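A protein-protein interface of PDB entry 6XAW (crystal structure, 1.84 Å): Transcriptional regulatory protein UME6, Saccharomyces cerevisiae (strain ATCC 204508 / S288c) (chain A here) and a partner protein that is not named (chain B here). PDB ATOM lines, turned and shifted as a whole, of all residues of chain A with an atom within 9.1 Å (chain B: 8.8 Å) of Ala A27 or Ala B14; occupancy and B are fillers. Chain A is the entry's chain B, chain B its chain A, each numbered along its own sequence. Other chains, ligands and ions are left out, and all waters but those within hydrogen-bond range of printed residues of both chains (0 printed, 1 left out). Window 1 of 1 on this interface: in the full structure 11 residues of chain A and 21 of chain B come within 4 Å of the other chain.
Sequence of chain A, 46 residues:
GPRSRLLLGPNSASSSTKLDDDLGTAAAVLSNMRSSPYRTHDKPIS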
ATOM      1  N   ASP A  20      20.282  17.539 -28.262  1.00  0.00           N
ATOM      2  CA  ASP A  20      18.864  17.811 -28.466  1.00  0.00           C
ATOM      3  C   ASP A  20      18.070  16.516 -28.593  1.00  0.00           C
ATOM      4  O   ASP A  20      16.847  16.532 -28.413  1.00  0.00           O
ATOM      5  CB  ASP A  20      18.650  18.684 -29.705  1.00  0.00           C
ATOM      6  CG  ASP A  20      19.007  17.966 -30.995  1.00  0.00           C
ATOM      7  OD1 ASP A  20      20.125  18.191 -31.512  1.00  0.00           O
ATOM      8  OD2 ASP A  20      18.174  17.173 -31.489  1.00  0.00           O
ATOM      9  N   ASP A  21      18.748  15.402 -28.908  1.00  0.00           N
ATOM     10  CA  ASP A  21      18.134  14.075 -28.848  1.00  0.00           C
ATOM     11  C   ASP A  21      17.673  13.742 -27.433  1.00  0.00           C
ATOM     12  O   ASP A  21      16.514  13.372 -27.212  1.00  0.00           O
ATOM     13  CB  ASP A  21      19.116  13.006 -29.325  1.00  0.00           C
ATOM     14  CG  ASP A  21      19.207  12.916 -30.837  1.00  0.00           C
ATOM     15  OD1 ASP A  21      18.435  13.607 -31.538  1.00  0.00           O
ATOM     16  OD2 ASP A  21      20.059  12.140 -31.319  1.00  0.00           O
ATOM     17  N   ASP A  22      18.595  13.812 -26.465  1.00  0.00           N
ATOM     18  CA  ASP A  22      18.248  13.516 -25.078  1.00  0.00           C
ATOM     19  C   ASP A  22      17.155  14.452 -24.584  1.00  0.00           C
ATOM     20  O   ASP A  22      16.285  14.051 -23.803  1.00  0.00           O
ATOM     21  CB  ASP A  22      19.490  13.634 -24.193  1.00  0.00           C
ATOM     22  CG  ASP A  22      20.449  12.477 -24.376  1.00  0.00           C
ATOM     23  OD1 ASP A  22      20.022  11.436 -24.923  1.00  0.00           O
ATOM     24  OD2 ASP A  22      21.628  12.606 -23.974  1.00  0.00           O
ATOM     25  N   LEU A  23      17.192  15.707 -25.029  1.00  0.00           N
ATOM     26  CA  LEU A  23      16.188  16.681 -24.627  1.00  0.00           C
ATOM     27  C   LEU A  23      14.814  16.307 -25.176  1.00  0.00           C
ATOM     28  O   LEU A  23      13.820  16.300 -24.435  1.00  0.00           O
ATOM     29  CB  LEU A  23      16.615  18.077 -25.097  1.00  0.00           C
ATOM     30  CG  LEU A  23      15.947  19.283 -24.432  1.00  0.00           C
ATOM     31  CD1 LEU A  23      16.785  20.540 -24.619  1.00  0.00           C
ATOM     32  CD2 LEU A  23      14.548  19.492 -24.997  1.00  0.00           C
ATOM     33  N   GLY A  24      14.734  16.012 -26.476  1.00  0.00           N
ATOM     34  CA  GLY A  24      13.462  15.619 -27.060  1.00  0.00           C
ATOM     35  C   GLY A  24      12.942  14.302 -26.505  1.00  0.00           C
ATOM     36  O   GLY A  24      11.734  14.128 -26.318  1.00  0.00           O
ATOM     37  N   THR A  25      13.845  13.362 -26.234  1.00  0.00           N
ATOM     38  CA  THR A  25      13.434  12.117 -25.587  1.00  0.00           C
ATOM     39  C   THR A  25      12.766  12.385 -24.244  1.00  0.00           C
ATOM     40  O   THR A  25      11.699  11.834 -23.950  1.00  0.00           O
ATOM     41  CB  THR A  25      14.640  11.202 -25.413  1.00  0.00           C
ATOM     42  OG1 THR A  25      15.049  10.743 -26.696  1.00  0.00           O
ATOM     43  CG2 THR A  25      14.285   9.994 -24.539  1.00  0.00           C
ATOM     44  N   ALA A  26      13.389  13.209 -23.399  1.00  0.00           N
ATOM     45  CA  ALA A  26      12.783  13.522 -22.108  1.00  0.00           C
ATOM     46  C   ALA A  26      11.445  14.234 -22.287  1.00  0.00           C
ATOM     47  O   ALA A  26      10.484  13.970 -21.556  1.00  0.00           O
ATOM     48  CB  ALA A  26      13.733  14.372 -21.274  1.00  0.00           C
ATOM     49  N   ALA A  27      11.362  15.138 -23.261  1.00  0.00           N
ATOM     50  CA  ALA A  27      10.107  15.836 -23.513  1.00  0.00           C
ATOM     51  C   ALA A  27       9.001  14.870 -23.904  1.00  0.00           C
ATOM     52  O   ALA A  27       7.854  15.029 -23.477  1.00  0.00           O
ATOM     53  CB  ALA A  27      10.294  16.884 -24.605  1.00  0.00           C
ATOM     54  N   ALA A  28       9.323  13.865 -24.724  1.00  0.00           N
ATOM     55  CA  ALA A  28       8.302  12.918 -25.152  1.00  0.00           C
ATOM     56  C   ALA A  28       7.767  12.122 -23.971  1.00  0.00           C
ATOM     57  O   ALA A  28       6.560  11.879 -23.870  1.00  0.00           O
ATOM     58  CB  ALA A  28       8.858  11.981 -26.220  1.00  0.00           C
ATOM     59  N   VAL A  29       8.655  11.706 -23.070  1.00  0.00           N
ATOM     60  CA  VAL A  29       8.224  10.947 -21.899  1.00  0.00           C
ATOM     61  C   VAL A  29       7.409  11.833 -20.967  1.00  0.00           C
ATOM     62  O   VAL A  29       6.321  11.459 -20.508  1.00  0.00           O
ATOM     63  CB  VAL A  29       9.450  10.350 -21.187  1.00  0.00           C
ATOM     64  CG1 VAL A  29       9.035   9.699 -19.851  1.00  0.00           C
ATOM     65  CG2 VAL A  29      10.147   9.345 -22.113  1.00  0.00           C
ATOM     66  N   LEU A  30       7.933  13.022 -20.669  1.00  0.00           N
ATOM     67  CA  LEU A  30       7.223  13.968 -19.823  1.00  0.00           C
ATOM     68  C   LEU A  30       5.829  14.256 -20.366  1.00  0.00           C
ATOM     69  O   LEU A  30       4.845  14.257 -19.616  1.00  0.00           O
ATOM     70  CB  LEU A  30       8.035  15.261 -19.718  1.00  0.00           C
ATOM     71  CG  LEU A  30       7.673  16.252 -18.629  1.00  0.00           C
ATOM     72  CD1 LEU A  30       7.694  15.594 -17.253  1.00  0.00           C
ATOM     73  CD2 LEU A  30       8.648  17.425 -18.702  1.00  0.00           C
ATOM     74  N   SER A  31       5.720  14.499 -21.675  1.00  0.00           N
ATOM     75  CA  SER A  31       4.462  14.993 -22.221  1.00  0.00           C
ATOM     76  C   SER A  31       3.406  13.905 -22.311  1.00  0.00           C
ATOM     77  O   SER A  31       2.242  14.211 -22.590  1.00  0.00           O
ATOM     78  CB  SER A  31       4.686  15.628 -23.598  1.00  0.00           C
ATOM     79  OG  SER A  31       4.926  14.654 -24.597  1.00  0.00           O
ATOM     80  N   ASN A  32       3.781  12.655 -22.059  1.00  0.00           N
ATOM     81  CA  ASN A  32       2.839  11.548 -22.046  1.00  0.00           C
ATOM     82  C   ASN A  32       2.533  11.011 -20.648  1.00  0.00           C
ATOM     83  O   ASN A  32       1.912   9.951 -20.541  1.00  0.00           O
ATOM     84  CB  ASN A  32       3.357  10.415 -22.932  1.00  0.00           C
ATOM     85  CG  ASN A  32       3.216  10.725 -24.409  1.00  0.00           C
ATOM     86  OD1 ASN A  32       2.166  11.184 -24.860  1.00  0.00           O
ATOM     87  ND2 ASN A  32       4.277  10.479 -25.171  1.00  0.00           N
ATOM     88  N   MET A  33       2.924  11.706 -19.570  1.00  0.00           N
ATOM     89  CA  MET A  33       2.502  11.183 -18.266  1.00  0.00           C
ATOM     90  C   MET A  33       1.050  11.525 -17.932  1.00  0.00           C
ATOM     91  O   MET A  33       0.412  10.803 -17.163  1.00  0.00           O
ATOM     92  CB  MET A  33       3.417  11.647 -17.122  1.00  0.00           C
ATOM     93  CG  MET A  33       4.911  11.648 -17.409  1.00  0.00           C
ATOM     94  SD  MET A  33       5.914  12.369 -16.088  1.00  0.00           S
ATOM     95  CE  MET A  33       6.060  10.974 -14.984  1.00  0.00           C
ATOM     96  N   ASP B   8       1.236  18.038 -28.574  1.00  0.00           N
ATOM     97  CA  ASP B   8       1.685  19.009 -29.580  1.00  0.00           C
ATOM     98  C   ASP B   8       2.069  20.355 -28.954  1.00  0.00           C
ATOM     99  O   ASP B   8       3.257  20.689 -28.904  1.00  0.00           O
ATOM    100  CB  ASP B   8       0.618  19.226 -30.641  1.00  0.00           C
ATOM    101  CG  ASP B   8       1.122  20.061 -31.794  1.00  0.00           C
ATOM    102  OD1 ASP B   8       0.306  20.766 -32.425  1.00  0.00           O
ATOM    103  OD2 ASP B   8       2.341  20.015 -32.062  1.00  0.00           O
ATOM    104  N   VAL B   9       1.082  21.142 -28.507  1.00  0.00           N
ATOM    105  CA  VAL B   9       1.399  22.233 -27.588  1.00  0.00           C
ATOM    106  C   VAL B   9       2.054  21.660 -26.331  1.00  0.00           C
ATOM    107  O   VAL B   9       3.081  22.157 -25.861  1.00  0.00           O
ATOM    108  CB  VAL B   9       0.144  23.056 -27.242  1.00  0.00           C
ATOM    109  CG1 VAL B   9       0.376  23.853 -25.970  1.00  0.00           C
ATOM    110  CG2 VAL B   9      -0.222  24.021 -28.380  1.00  0.00           C
ATOM    111  N   GLU B  10       1.483  20.575 -25.796  1.00  0.00           N
ATOM    112  CA  GLU B  10       2.051  19.965 -24.594  1.00  0.00           C
ATOM    113  C   GLU B  10       3.471  19.461 -24.841  1.00  0.00           C
ATOM    114  O   GLU B  10       4.345  19.584 -23.974  1.00  0.00           O
ATOM    115  CB  GLU B  10       1.153  18.818 -24.113  1.00  0.00           C
ATOM    116  CG  GLU B  10      -0.219  19.257 -23.626  1.00  0.00           C
ATOM    117  CD  GLU B  10      -1.158  19.606 -24.767  1.00  0.00           C
ATOM    118  OE1 GLU B  10      -2.152  20.318 -24.517  1.00  0.00           O
ATOM    119  OE2 GLU B  10      -0.895  19.178 -25.914  1.00  0.00           O
ATOM    120  N   PHE B  11       3.715  18.862 -26.005  1.00  0.00           N
ATOM    121  CA  PHE B  11       5.073  18.452 -26.339  1.00  0.00           C
ATOM    122  C   PHE B  11       6.007  19.653 -26.363  1.00  0.00           C
ATOM    123  O   PHE B  11       7.108  19.609 -25.800  1.00  0.00           O
ATOM    124  CB  PHE B  11       5.082  17.734 -27.681  1.00  0.00           C
ATOM    125  CG  PHE B  11       6.410  17.149 -28.051  1.00  0.00           C
ATOM    126  CD1 PHE B  11       6.905  16.050 -27.387  1.00  0.00           C
ATOM    127  CD2 PHE B  11       7.151  17.685 -29.090  1.00  0.00           C
ATOM    128  CE1 PHE B  11       8.124  15.497 -27.738  1.00  0.00           C
ATOM    129  CE2 PHE B  11       8.369  17.131 -29.445  1.00  0.00           C
ATOM    130  CZ  PHE B  11       8.858  16.037 -28.758  1.00  0.00           C
ATOM    131  N   SER B  12       5.571  20.752 -26.991  1.00  0.00           N
ATOM    132  CA  SER B  12       6.420  21.937 -27.036  1.00  0.00           C
ATOM    133  C   SER B  12       6.648  22.510 -25.648  1.00  0.00           C
ATOM    134  O   SER B  12       7.736  23.013 -25.345  1.00  0.00           O
ATOM    135  CB  SER B  12       5.796  22.992 -27.949  1.00  0.00           C
ATOM    136  OG  SER B  12       5.791  22.517 -29.276  1.00  0.00           O
ATOM    137  N   GLN B  13       5.629  22.457 -24.790  1.00  0.00           N
ATOM    138  CA  GLN B  13       5.807  22.941 -23.427  1.00  0.00           C
ATOM    139  C   GLN B  13       6.814  22.074 -22.682  1.00  0.00           C
ATOM    140  O   GLN B  13       7.642  22.585 -21.917  1.00  0.00           O
ATOM    141  CB  GLN B  13       4.461  22.967 -22.699  1.00  0.00           C
ATOM    142  CG  GLN B  13       3.523  24.079 -23.192  1.00  0.00           C
ATOM    143  CD  GLN B  13       2.119  23.949 -22.635  1.00  0.00           C
ATOM    144  OE1 GLN B  13       1.602  22.845 -22.499  1.00  0.00           O
ATOM    145  NE2 GLN B  13       1.488  25.082 -22.318  1.00  0.00           N
ATOM    146  N   ALA B  14       6.759  20.758 -22.905  1.00  0.00           N
ATOM    147  CA  ALA B  14       7.747  19.850 -22.320  1.00  0.00           C
ATOM    148  C   ALA B  14       9.157  20.150 -22.828  1.00  0.00           C
ATOM    149  O   ALA B  14      10.120  20.157 -22.049  1.00  0.00           O
ATOM    150  CB  ALA B  14       7.364  18.398 -22.622  1.00  0.00           C
ATOM    151  N   ILE B  15       9.303  20.396 -24.133  1.00  0.00           N
ATOM    152  CA  ILE B  15      10.617  20.737 -24.666  1.00  0.00           C
ATOM    153  C   ILE B  15      11.139  22.007 -24.004  1.00  0.00           C
ATOM    154  O   ILE B  15      12.309  22.090 -23.615  1.00  0.00           O
ATOM    155  CB  ILE B  15      10.556  20.891 -26.194  1.00  0.00           C
ATOM    156  CG1 ILE B  15      10.477  19.532 -26.877  1.00  0.00           C
ATOM    157  CG2 ILE B  15      11.769  21.637 -26.690  1.00  0.00           C
ATOM    158  CD1 ILE B  15      10.217  19.636 -28.346  1.00  0.00           C
ATOM    159  N   SER B  16      10.277  23.017 -23.867  1.00  0.00           N
ATOM    160  CA  SER B  16      10.701  24.269 -23.248  1.00  0.00           C
ATOM    161  C   SER B  16      11.091  24.059 -21.793  1.00  0.00           C
ATOM    162  O   SER B  16      12.083  24.630 -21.320  1.00  0.00           O
ATOM    163  CB  SER B  16       9.591  25.311 -23.367  1.00  0.00           C
ATOM    164  OG  SER B  16       9.244  25.477 -24.729  1.00  0.00           O
ATOM    165  N   TYR B  17      10.332  23.226 -21.077  1.00  0.00           N
ATOM    166  CA  TYR B  17      10.642  22.946 -19.680  1.00  0.00           C
ATOM    167  C   TYR B  17      11.975  22.218 -19.542  1.00  0.00           C
ATOM    168  O   TYR B  17      12.822  22.600 -18.723  1.00  0.00           O
ATOM    169  CB  TYR B  17       9.520  22.116 -19.053  1.00  0.00           C
ATOM    170  CG  TYR B  17       9.837  21.664 -17.642  1.00  0.00           C
ATOM    171  CD1 TYR B  17      10.114  22.587 -16.637  1.00  0.00           C
ATOM    172  CD2 TYR B  17       9.839  20.314 -17.308  1.00  0.00           C
ATOM    173  CE1 TYR B  17      10.406  22.160 -15.334  1.00  0.00           C
ATOM    174  CE2 TYR B  17      10.122  19.898 -16.038  1.00  0.00           C
ATOM    175  CZ  TYR B  17      10.411  20.822 -15.052  1.00  0.00           C
ATOM    176  OH  TYR B  17      10.692  20.406 -13.770  1.00  0.00           O
ATOM    177  N   VAL B  18      12.176  21.148 -20.313  1.00  0.00           N
ATOM    178  CA  VAL B  18      13.430  20.413 -20.177  1.00  0.00           C
ATOM    179  C   VAL B  18      14.608  21.306 -20.548  1.00  0.00           C
ATOM    180  O   VAL B  18      15.671  21.243 -19.919  1.00  0.00           O
ATOM    181  CB  VAL B  18      13.395  19.114 -21.006  1.00  0.00           C
ATOM    182  CG1 VAL B  18      14.747  18.400 -20.942  1.00  0.00           C
ATOM    183  CG2 VAL B  18      12.285  18.201 -20.509  1.00  0.00           C
ATOM    184  N   ASN B  19      14.432  22.201 -21.528  1.00  0.00           N
ATOM    185  CA  ASN B  19      15.506  23.145 -21.819  1.00  0.00           C
ATOM    186  C   ASN B  19      15.786  24.059 -20.631  1.00  0.00           C
ATOM    187  O   ASN B  19      16.937  24.445 -20.392  1.00  0.00           O
ATOM    188  CB  ASN B  19      15.170  23.994 -23.045  1.00  0.00           C
ATOM    189  CG  ASN B  19      16.350  24.815 -23.495  1.00  0.00           C
ATOM    190  OD1 ASN B  19      17.353  24.269 -23.955  1.00  0.00           O
ATOM    191  ND2 ASN B  19      16.259  26.131 -23.324  1.00  0.00           N
ATOM    192  N   LYS B  20      14.743  24.443 -19.894  1.00  0.00           N
ATOM    193  CA  LYS B  20      14.933  25.289 -18.725  1.00  0.00           C
ATOM    194  C   LYS B  20      15.766  24.566 -17.679  1.00  0.00           C
ATOM    195  O   LYS B  20      16.622  25.170 -17.024  1.00  0.00           O
ATOM    196  CB  LYS B  20      13.576  25.684 -18.149  1.00  0.00           C
ATOM    197  CG  LYS B  20      13.600  26.750 -17.067  1.00  0.00           C
ATOM    198  CD  LYS B  20      12.172  27.088 -16.634  1.00  0.00           C
ATOM    199  CE  LYS B  20      12.157  28.000 -15.405  1.00  0.00           C
ATOM    200  NZ  LYS B  20      10.802  28.109 -14.776  1.00  0.00           N
ATOM    201  N   ILE B  21      15.531  23.266 -17.520  1.00  0.00           N
ATOM    202  CA  ILE B  21      16.329  22.489 -16.578  1.00  0.00           C
ATOM    203  C   ILE B  21      17.774  22.436 -17.044  1.00  0.00           C
ATOM    204  O   ILE B  21      18.700  22.698 -16.274  1.00  0.00           O
ATOM    205  CB  ILE B  21      15.739  21.081 -16.407  1.00  0.00           C
ATOM    206  CG1 ILE B  21      14.340  21.158 -15.776  1.00  0.00           C
ATOM    207  CG2 ILE B  21      16.693  20.192 -15.558  1.00  0.00           C
ATOM    208  CD1 ILE B  21      13.576  19.842 -15.898  1.00  0.00           C
ATOM    209  N   TYR B  32      21.121  17.691 -14.398  1.00  0.00           N
ATOM    210  CA  TYR B  32      20.344  17.535 -15.623  1.00  0.00           C
ATOM    211  C   TYR B  32      20.315  16.079 -16.068  1.00  0.00           C
ATOM    212  O   TYR B  32      19.248  15.526 -16.385  1.00  0.00           O
ATOM    213  CB  TYR B  32      20.940  18.425 -16.719  1.00  0.00           C
ATOM    214  CG  TYR B  32      20.340  18.212 -18.087  1.00  0.00           C
ATOM    215  CD1 TYR B  32      18.981  18.440 -18.319  1.00  0.00           C
ATOM    216  CD2 TYR B  32      21.134  17.805 -19.162  1.00  0.00           C
ATOM    217  CE1 TYR B  32      18.427  18.256 -19.590  1.00  0.00           C
ATOM    218  CE2 TYR B  32      20.590  17.617 -20.425  1.00  0.00           C
ATOM    219  CZ  TYR B  32      19.238  17.842 -20.635  1.00  0.00           C
ATOM    220  OH  TYR B  32      18.702  17.660 -21.906  1.00  0.00           O
ATOM    221  N   PHE B  35      17.987  14.067 -13.955  1.00  0.00           N
ATOM    222  CA  PHE B  35      16.599  14.275 -14.356  1.00  0.00           C
ATOM    223  C   PHE B  35      16.253  13.434 -15.579  1.00  0.00           C
ATOM    224  O   PHE B  35      15.193  12.799 -15.629  1.00  0.00           O
ATOM    225  CB  PHE B  35      16.329  15.758 -14.650  1.00  0.00           C
ATOM    226  CG  PHE B  35      14.929  16.024 -15.125  1.00  0.00           C
ATOM    227  CD1 PHE B  35      13.883  16.125 -14.223  1.00  0.00           C
ATOM    228  CD2 PHE B  35      14.651  16.148 -16.481  1.00  0.00           C
ATOM    229  CE1 PHE B  35      12.582  16.366 -14.669  1.00  0.00           C
ATOM    230  CE2 PHE B  35      13.361  16.374 -16.921  1.00  0.00           C
ATOM    231  CZ  PHE B  35      12.334  16.483 -16.026  1.00  0.00           C
ATOM    232  N   LEU B  36      17.126  13.448 -16.590  1.00  0.00           N
ATOM    233  CA  LEU B  36      16.900  12.628 -17.771  1.00  0.00           C
ATOM    234  C   LEU B  36      16.754  11.157 -17.393  1.00  0.00           C
ATOM    235  O   LEU B  36      15.895  10.457 -17.929  1.00  0.00           O
ATOM    236  CB  LEU B  36      18.050  12.778 -18.757  1.00  0.00           C
ATOM    237  CG  LEU B  36      18.267  14.134 -19.426  1.00  0.00           C
ATOM    238  CD1 LEU B  36      19.411  14.010 -20.403  1.00  0.00           C
ATOM    239  CD2 LEU B  36      17.002  14.562 -20.116  1.00  0.00           C
ATOM    240  N   LEU B  39      13.405  10.085 -15.877  1.00  0.00           N
ATOM    241  CA  LEU B  39      12.380   9.829 -16.882  1.00  0.00           C
ATOM    242  C   LEU B  39      12.641   8.520 -17.624  1.00  0.00           C
ATOM    243  O   LEU B  39      11.703   7.772 -17.923  1.00  0.00           O
ATOM    244  CB  LEU B  39      12.295  11.002 -17.865  1.00  0.00           C
ATOM    245  CG  LEU B  39      11.833  12.311 -17.222  1.00  0.00           C
ATOM    246  CD1 LEU B  39      11.726  13.419 -18.268  1.00  0.00           C
ATOM    247  CD2 LEU B  39      10.511  12.111 -16.497  1.00  0.00           C
ATOM    248  N   GLN B  40      13.902   8.228 -17.943  1.00  0.00           N
ATOM    249  CA  GLN B  40      14.196   6.969 -18.629  1.00  0.00           C
ATOM    250  C   GLN B  40      13.854   5.774 -17.740  1.00  0.00           C
ATOM    251  O   GLN B  40      13.324   4.761 -18.216  1.00  0.00           O
ATOM    252  CB  GLN B  40      15.665   6.927 -19.048  1.00  0.00           C
ATOM    253  CG  GLN B  40      16.010   7.810 -20.271  1.00  0.00           C
ATOM    254  CD  GLN B  40      15.038   7.619 -21.436  1.00  0.00           C
ATOM    255  OE1 GLN B  40      14.042   8.332 -21.554  1.00  0.00           O
ATOM    256  NE2 GLN B  40      15.327   6.651 -22.294  1.00  0.00           N
ATOM    257  N   ASP B  69       6.835  23.697 -11.940  1.00  0.00           N
ATOM    258  CA  ASP B  69       6.667  23.511 -13.381  1.00  0.00           C
ATOM    259  C   ASP B  69       6.476  22.040 -13.726  1.00  0.00           C
ATOM    260  O   ASP B  69       5.670  21.694 -14.600  1.00  0.00           O
ATOM    261  CB  ASP B  69       7.885  24.035 -14.130  1.00  0.00           C
ATOM    262  CG  ASP B  69       7.959  25.545 -14.172  1.00  0.00           C
ATOM    263  OD1 ASP B  69       6.962  26.217 -13.831  1.00  0.00           O
ATOM    264  OD2 ASP B  69       9.037  26.049 -14.558  1.00  0.00           O
ATOM    265  N   PHE B  73       2.841  18.787 -15.653  1.00  0.00           N
ATOM    266  CA  PHE B  73       2.798  17.659 -16.572  1.00  0.00           C
ATOM    267  C   PHE B  73       2.142  16.418 -15.970  1.00  0.00           C
ATOM    268  O   PHE B  73       1.934  15.438 -16.692  1.00  0.00           O
ATOM    269  CB  PHE B  73       4.215  17.345 -17.064  1.00  0.00           C
ATOM    270  CG  PHE B  73       4.810  18.478 -17.865  1.00  0.00           C
ATOM    271  CD1 PHE B  73       5.603  19.432 -17.248  1.00  0.00           C
ATOM    272  CD2 PHE B  73       4.508  18.626 -19.217  1.00  0.00           C
ATOM    273  CE1 PHE B  73       6.123  20.514 -17.969  1.00  0.00           C
ATOM    274  CE2 PHE B  73       5.028  19.703 -19.951  1.00  0.00           C
ATOM    275  CZ  PHE B  73       5.830  20.650 -19.321  1.00  0.00           C
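Of the 14 printed residues of chain A, 9 touch a printed residue of chain B. Hydrophobic or aromatic side chains of chain A within 4 Å of the printed part of chain B: Leu A23, Ala A26, Ala A27, Ala A28, Val A29 and Leu A30. Printed residues of chain B that touch a printed residue of chain A: Glu B10, Phe B11, Ala B14, Ile B15, Tyr B17, Val B18, Asn B19, Tyr B32, Leu B36, Leu B39, Gln B40 and Phe B73. Among the printed residues, 18 pairs touch across the chains. Among the printed residues, no Asp or Glu carboxylate lies within 4 Å of a Lys or Arg side-chain nitrogen of the other chain.
O of Asp A22 touches CD2 of Leu B36 (3.8 Å). O of Ile B15 touches CD2 of Leu A23 (3.7 Å). CG1 of Val B18 touches CG of Leu A23, 3.8 Å away. Asn B19 touches Leu A23 (OD1 to CD1, 3.8 Å). CD1 of Leu B39 touches O of Ala A26, at 3.6 Å. CE1 of Phe B11 touches C of Ala A27 (3.98 Å). Ala A27 touches Ile B15 (CB to CG1, 3.5 Å). Ala A28 touches Phe B11. Ser A31 touches Glu B10 (CB to O, 3.99 Å). Ser A31 touches Phe B11.
No residue of chain B comes within 4 Å of Gly A24. Ala A26 touches just these residues of chain B: Leu B36 and Leu B39. Ala A28 touches just one residue of chain B: Phe B11. Printed residues of chain A within 4 Å of Leu B36: Asp A22 (3.8 Å) and Ala A26 (3.5 Å). Printed residues of chain A within 4 Å of Tyr B17: Leu A30. Of the printed residues of chain A, Glu B10 touches Ser A31. Printed residues of chain A within 4 Å of Leu B39: Ala A26 (3.6 Å) and Val A29 (3.8 Å). Asp B69 touches none of the printed residues of chain A. The nearest printed residue of chain B that does not touch Ala A27 is Val B18 (4.2 Å). The nearest printed residue of chain B that does not touch Leu A30 is Val B18 (4.1 Å).
The backbone carbonyl oxygen (O) of Ala A27 lies within hydrogen-bond range of the side-chain hydroxyl (OG) of Ser A31, at 3.2 Å. The backbone carbonyl oxygen (O) of Ala A28 sits at hydrogen-bond distance from the side-chain amide nitrogen (ND2) of Asn A32, 3.0 Å away. The side-chain hydroxyl (OG) of Ser A31 sits at hydrogen-bond distance from the backbone carbonyl oxygen (O) of Ala A28 (3.3 Å). O of Asp A21 is in hydrogen-bond range of OG1 of Thr A25.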
